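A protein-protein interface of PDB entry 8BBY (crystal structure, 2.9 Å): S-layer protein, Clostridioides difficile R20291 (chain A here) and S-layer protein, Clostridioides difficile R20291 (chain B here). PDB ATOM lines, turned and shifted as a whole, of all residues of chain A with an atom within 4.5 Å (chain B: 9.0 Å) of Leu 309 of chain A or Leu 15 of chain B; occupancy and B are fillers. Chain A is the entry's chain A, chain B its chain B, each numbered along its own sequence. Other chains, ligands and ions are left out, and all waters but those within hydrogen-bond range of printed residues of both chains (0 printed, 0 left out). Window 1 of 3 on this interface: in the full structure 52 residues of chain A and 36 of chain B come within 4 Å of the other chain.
Of the 18 printed residues of chain B, 10 touch a printed residue of chain A.
Printed residues of chain B that touch a printed residue of chain A: Ala 7, Ser 11, Val 13, Lys 14, Leu 15, Thr 16, Leu 17, Val 29, Leu 32 and Arg 33.
Hydrophobic or aromatic side chains of chain B that line the printed part of chain A: Ala 7, Val 13, Leu 15, Leu 17, Val 29 and Leu 32.
Hydrophobic or aromatic side chains of chain A that line the printed part of chain B: Phe 275, Leu 280, Leu 283, Val 307, Val 308, Leu 309, Tyr 310 and Pro 311.
Along chain A the printed residues that touch a printed residue of chain B span positions 254 to 311.
O of Asp 8 of chain B lies within hydrogen-bond range of OG of Ser 11 of chain B, 3.3 Å away.
The guanidinium group (NE) of Arg 33 of chain B is in salt-bridge range of the side-chain carboxylate (OD1) of Asp 30 of chain B (2.8 Å).
Among the printed residues, merely in contact across the chains: Glu 254 of chain A with Leu 15 of chain B, Pro 311 of chain A with Val 13 of chain B, Tyr 310 of chain A with Lys 14 of chain B, Leu 280 of chain A with Val 29 of chain B, Tyr 310 of chain A with Ala 7 of chain B, Val 308 of chain A with Leu 15 of chain B, Val 307 of chain A with Thr 16 of chain B, Pro 311 of chain A with Leu 15 of chain B, Phe 275 of chain A with Leu 32 of chain B, Leu 280 of chain A with Arg 33 of chain B, Tyr 310 of chain A with Val 13 of chain B, Leu 309 of chain A with Lys 14 of chain B, Leu 283 of chain A with Val 29 of chain B, Leu 280 of chain A with Leu 32 of chain B, Leu 309 of chain A with Leu 17 of chain B, Glu 254 of chain A with Val 13 of chain B, Tyr 310 of chain A with Ser 11 of chain B and Val 308 of chain A with Thr 16 of chain B.
The backbone NH of Glu 254 of chain A sits at hydrogen-bond distance from the backbone carbonyl oxygen of Lys 14 of chain B (3.3 Å).
The backbone carbonyl oxygen (O) of Glu 254 of chain A is in hydrogen-bond range of the backbone NH (N) of Thr 16 of chain B.
The backbone carbonyl oxygen (O) of Val 307 of chain A sits at hydrogen-bond distance from the backbone NH (N) of Leu 17 of chain B, at 2.7 Å.
The backbone NH (N) of Leu 309 of chain A lies within hydrogen-bond range of the backbone carbonyl oxygen (O) of Leu 15 of chain B, 2.6 Å away.
OG of Ser 11 of chain B is in hydrogen-bond range of O of Pro 311 of chain A (2.5 Å).
Of the printed residues of chain B, Leu 280 of chain A touches Val 29, Leu 32 and Arg 33.
Printed residues of chain B within 4 Å of Val 307 of chain A: Thr 16 (3.4 Å) and Leu 17 (2.7 Å).
Leu 309 of chain A touches just these residues of chain B: Lys 14 (3.8 Å), Leu 15 (2.6 Å) and Leu 17 (3.8 Å).
Pro 12 of chain B touches none of the printed residues of chain A.
Of chain A, only Glu 254 (3.1 Å), Val 308 (3.4 Å), Leu 309 (2.6 Å) and Pro 311 (3.5 Å) come within 4 Å of Leu 15 of chain B.
Leu 25 of chain B touches none of the printed residues of chain A.
Printed residues of chain A within 4 Å of Arg 33 of chain B: Leu 280.
The nearest residue of chain A that does not touch Leu 15 of chain B is Val 307 of chain A (4.05 Å).
The nearest printed residue of chain B that does not touch Leu 283 of chain A is Leu 25 of chain B (5.9 Å).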
ATOM      1  N   GLU A 254      -0.028 -30.213  12.894  1.00  0.00           N
ATOM      2  CA  GLU A 254      -0.470 -29.257  13.906  1.00  0.00           C
ATOM      3  C   GLU A 254      -1.773 -28.631  13.426  1.00  0.00           C
ATOM      4  O   GLU A 254      -1.773 -27.884  12.445  1.00  0.00           O
ATOM      5  CB  GLU A 254       0.595 -28.195  14.153  1.00  0.00           C
ATOM      6  CG  GLU A 254       0.473 -27.494  15.495  1.00  0.00           C
ATOM      7  CD  GLU A 254       1.804 -26.978  16.006  1.00  0.00           C
ATOM      8  OE1 GLU A 254       2.051 -25.758  15.900  1.00  0.00           O
ATOM      9  OE2 GLU A 254       2.604 -27.793  16.510  1.00  0.00           O
ATOM     10  N   PHE A 275       4.846 -16.945   6.815  1.00  0.00           N
ATOM     11  CA  PHE A 275       3.848 -17.464   5.893  1.00  0.00           C
ATOM     12  C   PHE A 275       4.010 -16.842   4.513  1.00  0.00           C
ATOM     13  O   PHE A 275       4.540 -15.736   4.367  1.00  0.00           O
ATOM     14  CB  PHE A 275       2.430 -17.195   6.410  1.00  0.00           C
ATOM     15  CG  PHE A 275       2.076 -17.974   7.643  1.00  0.00           C
ATOM     16  CD1 PHE A 275       1.629 -19.281   7.547  1.00  0.00           C
ATOM     17  CD2 PHE A 275       2.188 -17.399   8.898  1.00  0.00           C
ATOM     18  CE1 PHE A 275       1.301 -20.001   8.680  1.00  0.00           C
ATOM     19  CE2 PHE A 275       1.862 -18.113  10.034  1.00  0.00           C
ATOM     20  CZ  PHE A 275       1.418 -19.417   9.925  1.00  0.00           C
ATOM     21  N   LEU A 280      -1.963 -16.838   1.038  1.00  0.00           N
ATOM     22  CA  LEU A 280      -2.974 -16.267   1.919  1.00  0.00           C
ATOM     23  C   LEU A 280      -3.921 -15.344   1.163  1.00  0.00           C
ATOM     24  O   LEU A 280      -5.077 -15.178   1.569  1.00  0.00           O
ATOM     25  CB  LEU A 280      -2.304 -15.514   3.068  1.00  0.00           C
ATOM     26  CG  LEU A 280      -1.557 -16.375   4.087  1.00  0.00           C
ATOM     27  CD1 LEU A 280      -0.928 -15.513   5.169  1.00  0.00           C
ATOM     28  CD2 LEU A 280      -2.489 -17.408   4.697  1.00  0.00           C
ATOM     29  N   LEU A 283      -6.360 -17.511  -1.066  1.00  0.00           N
ATOM     30  CA  LEU A 283      -7.246 -18.208  -0.142  1.00  0.00           C
ATOM     31  C   LEU A 283      -8.363 -17.291   0.336  1.00  0.00           C
ATOM     32  O   LEU A 283      -9.525 -17.706   0.415  1.00  0.00           O
ATOM     33  CB  LEU A 283      -6.446 -18.751   1.040  1.00  0.00           C
ATOM     34  CG  LEU A 283      -7.236 -19.468   2.134  1.00  0.00           C
ATOM     35  CD1 LEU A 283      -8.048 -20.601   1.533  1.00  0.00           C
ATOM     36  CD2 LEU A 283      -6.300 -19.989   3.215  1.00  0.00           C
ATOM     37  N   VAL A 307      -9.215 -25.266   5.885  1.00  0.00           N
ATOM     38  CA  VAL A 307      -8.161 -24.984   4.917  1.00  0.00           C
ATOM     39  C   VAL A 307      -6.848 -25.497   5.493  1.00  0.00           C
ATOM     40  O   VAL A 307      -6.682 -25.603   6.712  1.00  0.00           O
ATOM     41  CB  VAL A 307      -8.054 -23.480   4.579  1.00  0.00           C
ATOM     42  CG1 VAL A 307      -9.325 -22.987   3.905  1.00  0.00           C
ATOM     43  CG2 VAL A 307      -7.761 -22.671   5.830  1.00  0.00           C
ATOM     44  N   VAL A 308      -5.909 -25.817   4.607  1.00  0.00           N
ATOM     45  CA  VAL A 308      -4.587 -26.301   4.990  1.00  0.00           C
ATOM     46  C   VAL A 308      -3.568 -25.219   4.663  1.00  0.00           C
ATOM     47  O   VAL A 308      -3.604 -24.631   3.575  1.00  0.00           O
ATOM     48  CB  VAL A 308      -4.237 -27.622   4.280  1.00  0.00           C
ATOM     49  CG1 VAL A 308      -4.853 -28.799   5.020  1.00  0.00           C
ATOM     50  CG2 VAL A 308      -4.707 -27.590   2.833  1.00  0.00           C
ATOM     51  N   LEU A 309      -2.670 -24.949   5.609  1.00  0.00           N
ATOM     52  CA  LEU A 309      -1.658 -23.915   5.435  1.00  0.00           C
ATOM     53  C   LEU A 309      -0.307 -24.439   5.899  1.00  0.00           C
ATOM     54  O   LEU A 309      -0.204 -25.036   6.974  1.00  0.00           O
ATOM     55  CB  LEU A 309      -2.029 -22.644   6.207  1.00  0.00           C
ATOM     56  CG  LEU A 309      -3.024 -21.716   5.506  1.00  0.00           C
ATOM     57  CD1 LEU A 309      -3.520 -20.634   6.454  1.00  0.00           C
ATOM     58  CD2 LEU A 309      -2.400 -21.101   4.262  1.00  0.00           C
ATOM     59  N   TYR A 310       0.721 -24.209   5.085  1.00  0.00           N
ATOM     60  CA  TYR A 310       2.085 -24.606   5.400  1.00  0.00           C
ATOM     61  C   TYR A 310       2.945 -23.363   5.563  1.00  0.00           C
ATOM     62  O   TYR A 310       2.996 -22.538   4.637  1.00  0.00           O
ATOM     63  CB  TYR A 310       2.659 -25.492   4.298  1.00  0.00           C
ATOM     64  CG  TYR A 310       2.127 -26.906   4.242  1.00  0.00           C
ATOM     65  CD1 TYR A 310       0.962 -27.203   3.546  1.00  0.00           C
ATOM     66  CD2 TYR A 310       2.812 -27.952   4.846  1.00  0.00           C
ATOM     67  CE1 TYR A 310       0.481 -28.498   3.476  1.00  0.00           C
ATOM     68  CE2 TYR A 310       2.343 -29.249   4.778  1.00  0.00           C
ATOM     69  CZ  TYR A 310       1.176 -29.516   4.092  1.00  0.00           C
ATOM     70  OH  TYR A 310       0.704 -30.807   4.027  1.00  0.00           O
ATOM     71  N   PRO A 311       3.637 -23.176   6.687  1.00  0.00           N
ATOM     72  CA  PRO A 311       4.590 -22.064   6.778  1.00  0.00           C
ATOM     73  C   PRO A 311       5.825 -22.338   5.938  1.00  0.00           C
ATOM     74  O   PRO A 311       5.939 -23.398   5.315  1.00  0.00           O
ATOM     75  CB  PRO A 311       4.935 -22.000   8.273  1.00  0.00           C
ATOM     76  CG  PRO A 311       4.021 -22.968   8.952  1.00  0.00           C
ATOM     77  CD  PRO A 311       3.602 -23.966   7.925  1.00  0.00           C
ATOM     78  N   ALA B   4      -3.581 -26.967  -4.560  1.00  0.00           N
ATOM     79  CA  ALA B   4      -3.047 -25.697  -4.093  1.00  0.00           C
ATOM     80  C   ALA B   4      -1.546 -25.672  -4.342  1.00  0.00           C
ATOM     81  O   ALA B   4      -0.974 -26.600  -4.921  1.00  0.00           O
ATOM     82  CB  ALA B   4      -3.368 -25.473  -2.611  1.00  0.00           C
ATOM     83  N   SER B   5      -0.903 -24.592  -3.906  1.00  0.00           N
ATOM     84  CA  SER B   5       0.543 -24.489  -4.028  1.00  0.00           C
ATOM     85  C   SER B   5       1.213 -25.448  -3.053  1.00  0.00           C
ATOM     86  O   SER B   5       0.898 -25.456  -1.860  1.00  0.00           O
ATOM     87  CB  SER B   5       1.000 -23.056  -3.762  1.00  0.00           C
ATOM     88  OG  SER B   5       0.565 -22.185  -4.791  1.00  0.00           O
ATOM     89  N   ALA B   7       4.053 -27.251  -0.685  1.00  0.00           N
ATOM     90  CA  ALA B   7       4.757 -26.635   0.426  1.00  0.00           C
ATOM     91  C   ALA B   7       6.271 -26.721   0.253  1.00  0.00           C
ATOM     92  O   ALA B   7       6.794 -27.423  -0.617  1.00  0.00           O
ATOM     93  CB  ALA B   7       4.349 -27.294   1.741  1.00  0.00           C
ATOM     94  N   ASP B   8       6.977 -25.993   1.114  1.00  0.00           N
ATOM     95  CA  ASP B   8       8.431 -26.019   1.132  1.00  0.00           C
ATOM     96  C   ASP B   8       8.939 -27.250   1.873  1.00  0.00           C
ATOM     97  O   ASP B   8       8.266 -27.799   2.750  1.00  0.00           O
ATOM     98  CB  ASP B   8       8.984 -24.753   1.788  1.00  0.00           C
ATOM     99  CG  ASP B   8      10.483 -24.605   1.596  1.00  0.00           C
ATOM    100  OD1 ASP B   8      10.942 -24.619   0.434  1.00  0.00           O
ATOM    101  OD2 ASP B   8      11.203 -24.478   2.609  1.00  0.00           O
ATOM    102  N   SER B  11       9.363 -26.852   5.678  1.00  0.00           N
ATOM    103  CA  SER B  11       8.172 -26.414   6.389  1.00  0.00           C
ATOM    104  C   SER B  11       8.134 -27.068   7.765  1.00  0.00           C
ATOM    105  O   SER B  11       8.200 -28.304   7.856  1.00  0.00           O
ATOM    106  CB  SER B  11       6.914 -26.765   5.599  1.00  0.00           C
ATOM    107  OG  SER B  11       6.582 -25.737   4.682  1.00  0.00           O
ATOM    108  N   PRO B  12       8.043 -26.295   8.850  1.00  0.00           N
ATOM    109  CA  PRO B  12       8.100 -26.919  10.181  1.00  0.00           C
ATOM    110  C   PRO B  12       6.856 -27.716  10.524  1.00  0.00           C
ATOM    111  O   PRO B  12       6.963 -28.776  11.153  1.00  0.00           O
ATOM    112  CB  PRO B  12       8.286 -25.720  11.127  1.00  0.00           C
ATOM    113  CG  PRO B  12       8.615 -24.546  10.242  1.00  0.00           C
ATOM    114  CD  PRO B  12       7.973 -24.828   8.927  1.00  0.00           C
ATOM    115  N   VAL B  13       5.674 -27.242  10.128  1.00  0.00           N
ATOM    116  CA  VAL B  13       4.412 -27.862  10.508  1.00  0.00           C
ATOM    117  C   VAL B  13       3.433 -27.782   9.343  1.00  0.00           C
ATOM    118  O   VAL B  13       3.667 -27.099   8.345  1.00  0.00           O
ATOM    119  CB  VAL B  13       3.801 -27.208  11.766  1.00  0.00           C
ATOM    120  CG1 VAL B  13       4.427 -27.787  13.025  1.00  0.00           C
ATOM    121  CG2 VAL B  13       3.994 -25.705  11.719  1.00  0.00           C
ATOM    122  N   LYS B  14       2.327 -28.508   9.484  1.00  0.00           N
ATOM    123  CA  LYS B  14       1.196 -28.453   8.560  1.00  0.00           C
ATOM    124  C   LYS B  14      -0.016 -27.951   9.338  1.00  0.00           C
ATOM    125  O   LYS B  14      -0.668 -28.725  10.046  1.00  0.00           O
ATOM    126  CB  LYS B  14       0.920 -29.817   7.934  1.00  0.00           C
ATOM    127  CG  LYS B  14      -0.299 -29.831   7.023  1.00  0.00           C
ATOM    128  CD  LYS B  14      -1.101 -31.116   7.161  1.00  0.00           C
ATOM    129  CE  LYS B  14      -1.857 -31.420   5.876  1.00  0.00           C
ATOM    130  NZ  LYS B  14      -2.853 -32.515   6.042  1.00  0.00           N
ATOM    131  N   LEU B  15      -0.320 -26.663   9.210  1.00  0.00           N
ATOM    132  CA  LEU B  15      -1.464 -26.092   9.907  1.00  0.00           C
ATOM    133  C   LEU B  15      -2.751 -26.387   9.151  1.00  0.00           C
ATOM    134  O   LEU B  15      -2.862 -26.098   7.956  1.00  0.00           O
ATOM    135  CB  LEU B  15      -1.301 -24.582  10.089  1.00  0.00           C
ATOM    136  CG  LEU B  15      -0.281 -24.083  11.112  1.00  0.00           C
ATOM    137  CD1 LEU B  15      -0.259 -24.966  12.351  1.00  0.00           C
ATOM    138  CD2 LEU B  15       1.091 -23.985  10.494  1.00  0.00           C
ATOM    139  N   THR B  16      -3.720 -26.963   9.854  1.00  0.00           N
ATOM    140  CA  THR B  16      -5.075 -27.129   9.348  1.00  0.00           C
ATOM    141  C   THR B  16      -5.978 -26.165  10.106  1.00  0.00           C
ATOM    142  O   THR B  16      -6.129 -26.280  11.327  1.00  0.00           O
ATOM    143  CB  THR B  16      -5.562 -28.567   9.513  1.00  0.00           C
ATOM    144  OG1 THR B  16      -4.604 -29.466   8.938  1.00  0.00           O
ATOM    145  CG2 THR B  16      -6.903 -28.753   8.821  1.00  0.00           C
ATOM    146  N   LEU B  17      -6.563 -25.216   9.384  1.00  0.00           N
ATOM    147  CA  LEU B  17      -7.402 -24.183   9.976  1.00  0.00           C
ATOM    148  C   LEU B  17      -8.861 -24.553   9.751  1.00  0.00           C
ATOM    149  O   LEU B  17      -9.316 -24.623   8.605  1.00  0.00           O
ATOM    150  CB  LEU B  17      -7.093 -22.814   9.369  1.00  0.00           C
ATOM    151  CG  LEU B  17      -5.885 -22.045   9.912  1.00  0.00           C
ATOM    152  CD1 LEU B  17      -4.575 -22.697   9.498  1.00  0.00           C
ATOM    153  CD2 LEU B  17      -5.930 -20.597   9.454  1.00  0.00           C
ATOM    154  N   LYS B  18      -9.590 -24.783  10.840  1.00  0.00           N
ATOM    155  CA  LYS B  18     -10.979 -25.208  10.775  1.00  0.00           C
ATOM    156  C   LYS B  18     -11.868 -24.203  11.493  1.00  0.00           C
ATOM    157  O   LYS B  18     -11.468 -23.597  12.492  1.00  0.00           O
ATOM    158  CB  LYS B  18     -11.166 -26.601  11.391  1.00  0.00           C
ATOM    159  CG  LYS B  18     -10.409 -26.813  12.693  1.00  0.00           C
ATOM    160  CD  LYS B  18     -11.015 -27.942  13.512  1.00  0.00           C
ATOM    161  CE  LYS B  18      -9.938 -28.824  14.124  1.00  0.00           C
ATOM    162  NZ  LYS B  18     -10.511 -29.957  14.903  1.00  0.00           N
ATOM    163  N   LEU B  25     -13.111 -17.950   9.329  1.00  0.00           N
ATOM    164  CA  LEU B  25     -11.763 -18.269   8.879  1.00  0.00           C
ATOM    165  C   LEU B  25     -11.299 -17.358   7.751  1.00  0.00           C
ATOM    166  O   LEU B  25     -10.089 -17.210   7.551  1.00  0.00           O
ATOM    167  CB  LEU B  25     -11.673 -19.740   8.458  1.00  0.00           C
ATOM    168  CG  LEU B  25     -12.568 -20.311   7.361  1.00  0.00           C
ATOM    169  CD1 LEU B  25     -11.762 -20.467   6.098  1.00  0.00           C
ATOM    170  CD2 LEU B  25     -13.150 -21.647   7.780  1.00  0.00           C
ATOM    171  N   TYR B  28      -9.822 -14.729   9.814  1.00  0.00           N
ATOM    172  CA  TYR B  28      -8.557 -15.175  10.391  1.00  0.00           C
ATOM    173  C   TYR B  28      -7.436 -15.138   9.359  1.00  0.00           C
ATOM    174  O   TYR B  28      -6.299 -14.775   9.684  1.00  0.00           O
ATOM    175  CB  TYR B  28      -8.706 -16.579  10.975  1.00  0.00           C
ATOM    176  CG  TYR B  28      -7.590 -16.963  11.921  1.00  0.00           C
ATOM    177  CD1 TYR B  28      -6.433 -17.574  11.452  1.00  0.00           C
ATOM    178  CD2 TYR B  28      -7.689 -16.707  13.284  1.00  0.00           C
ATOM    179  CE1 TYR B  28      -5.409 -17.924  12.312  1.00  0.00           C
ATOM    180  CE2 TYR B  28      -6.669 -17.054  14.152  1.00  0.00           C
ATOM    181  CZ  TYR B  28      -5.533 -17.662  13.661  1.00  0.00           C
ATOM    182  OH  TYR B  28      -4.516 -18.008  14.522  1.00  0.00           O
ATOM    183  N   VAL B  29      -7.734 -15.518   8.116  1.00  0.00           N
ATOM    184  CA  VAL B  29      -6.740 -15.419   7.051  1.00  0.00           C
ATOM    185  C   VAL B  29      -6.380 -13.959   6.798  1.00  0.00           C
ATOM    186  O   VAL B  29      -5.213 -13.624   6.556  1.00  0.00           O
ATOM    187  CB  VAL B  29      -7.251 -16.116   5.777  1.00  0.00           C
ATOM    188  CG1 VAL B  29      -6.392 -15.748   4.577  1.00  0.00           C
ATOM    189  CG2 VAL B  29      -7.272 -17.623   5.971  1.00  0.00           C
ATOM    190  N   ASP B  30      -7.372 -13.067   6.852  1.00  0.00           N
ATOM    191  CA  ASP B  30      -7.102 -11.641   6.703  1.00  0.00           C
ATOM    192  C   ASP B  30      -6.204 -11.130   7.823  1.00  0.00           C
ATOM    193  O   ASP B  30      -5.247 -10.385   7.580  1.00  0.00           O
ATOM    194  CB  ASP B  30      -8.418 -10.861   6.673  1.00  0.00           C
ATOM    195  CG  ASP B  30      -8.397  -9.720   5.678  1.00  0.00           C
ATOM    196  OD1 ASP B  30      -7.293  -9.329   5.242  1.00  0.00           O
ATOM    197  OD2 ASP B  30      -9.484  -9.210   5.336  1.00  0.00           O
ATOM    198  N   LEU B  32      -4.168 -12.963   9.657  1.00  0.00           N
ATOM    199  CA  LEU B  32      -2.869 -13.622   9.571  1.00  0.00           C
ATOM    200  C   LEU B  32      -1.965 -12.935   8.556  1.00  0.00           C
ATOM    201  O   LEU B  32      -0.801 -12.636   8.847  1.00  0.00           O
ATOM    202  CB  LEU B  32      -3.052 -15.097   9.215  1.00  0.00           C
ATOM    203  CG  LEU B  32      -1.769 -15.927   9.133  1.00  0.00           C
ATOM    204  CD1 LEU B  32      -1.183 -16.158  10.520  1.00  0.00           C
ATOM    205  CD2 LEU B  32      -2.028 -17.251   8.427  1.00  0.00           C
ATOM    206  N   ARG B  33      -2.488 -12.667   7.356  1.00  0.00           N
ATOM    207  CA  ARG B  33      -1.664 -12.075   6.307  1.00  0.00           C
ATOM    208  C   ARG B  33      -1.225 -10.659   6.657  1.00  0.00           C
ATOM    209  O   ARG B  33      -0.186 -10.199   6.173  1.00  0.00           O
ATOM    210  CB  ARG B  33      -2.414 -12.089   4.974  1.00  0.00           C
ATOM    211  CG  ARG B  33      -3.482 -11.015   4.834  1.00  0.00           C
ATOM    212  CD  ARG B  33      -4.088 -11.018   3.439  1.00  0.00           C
ATOM    213  NE  ARG B  33      -5.424 -10.434   3.417  1.00  0.00           N
ATOM    214  CZ  ARG B  33      -6.180 -10.331   2.333  1.00  0.00           C
ATOM    215  NH1 ARG B  33      -5.762 -10.765   1.155  1.00  0.00           N
ATOM    216  NH2 ARG B  33      -7.386  -9.778   2.432  1.00  0.00           N
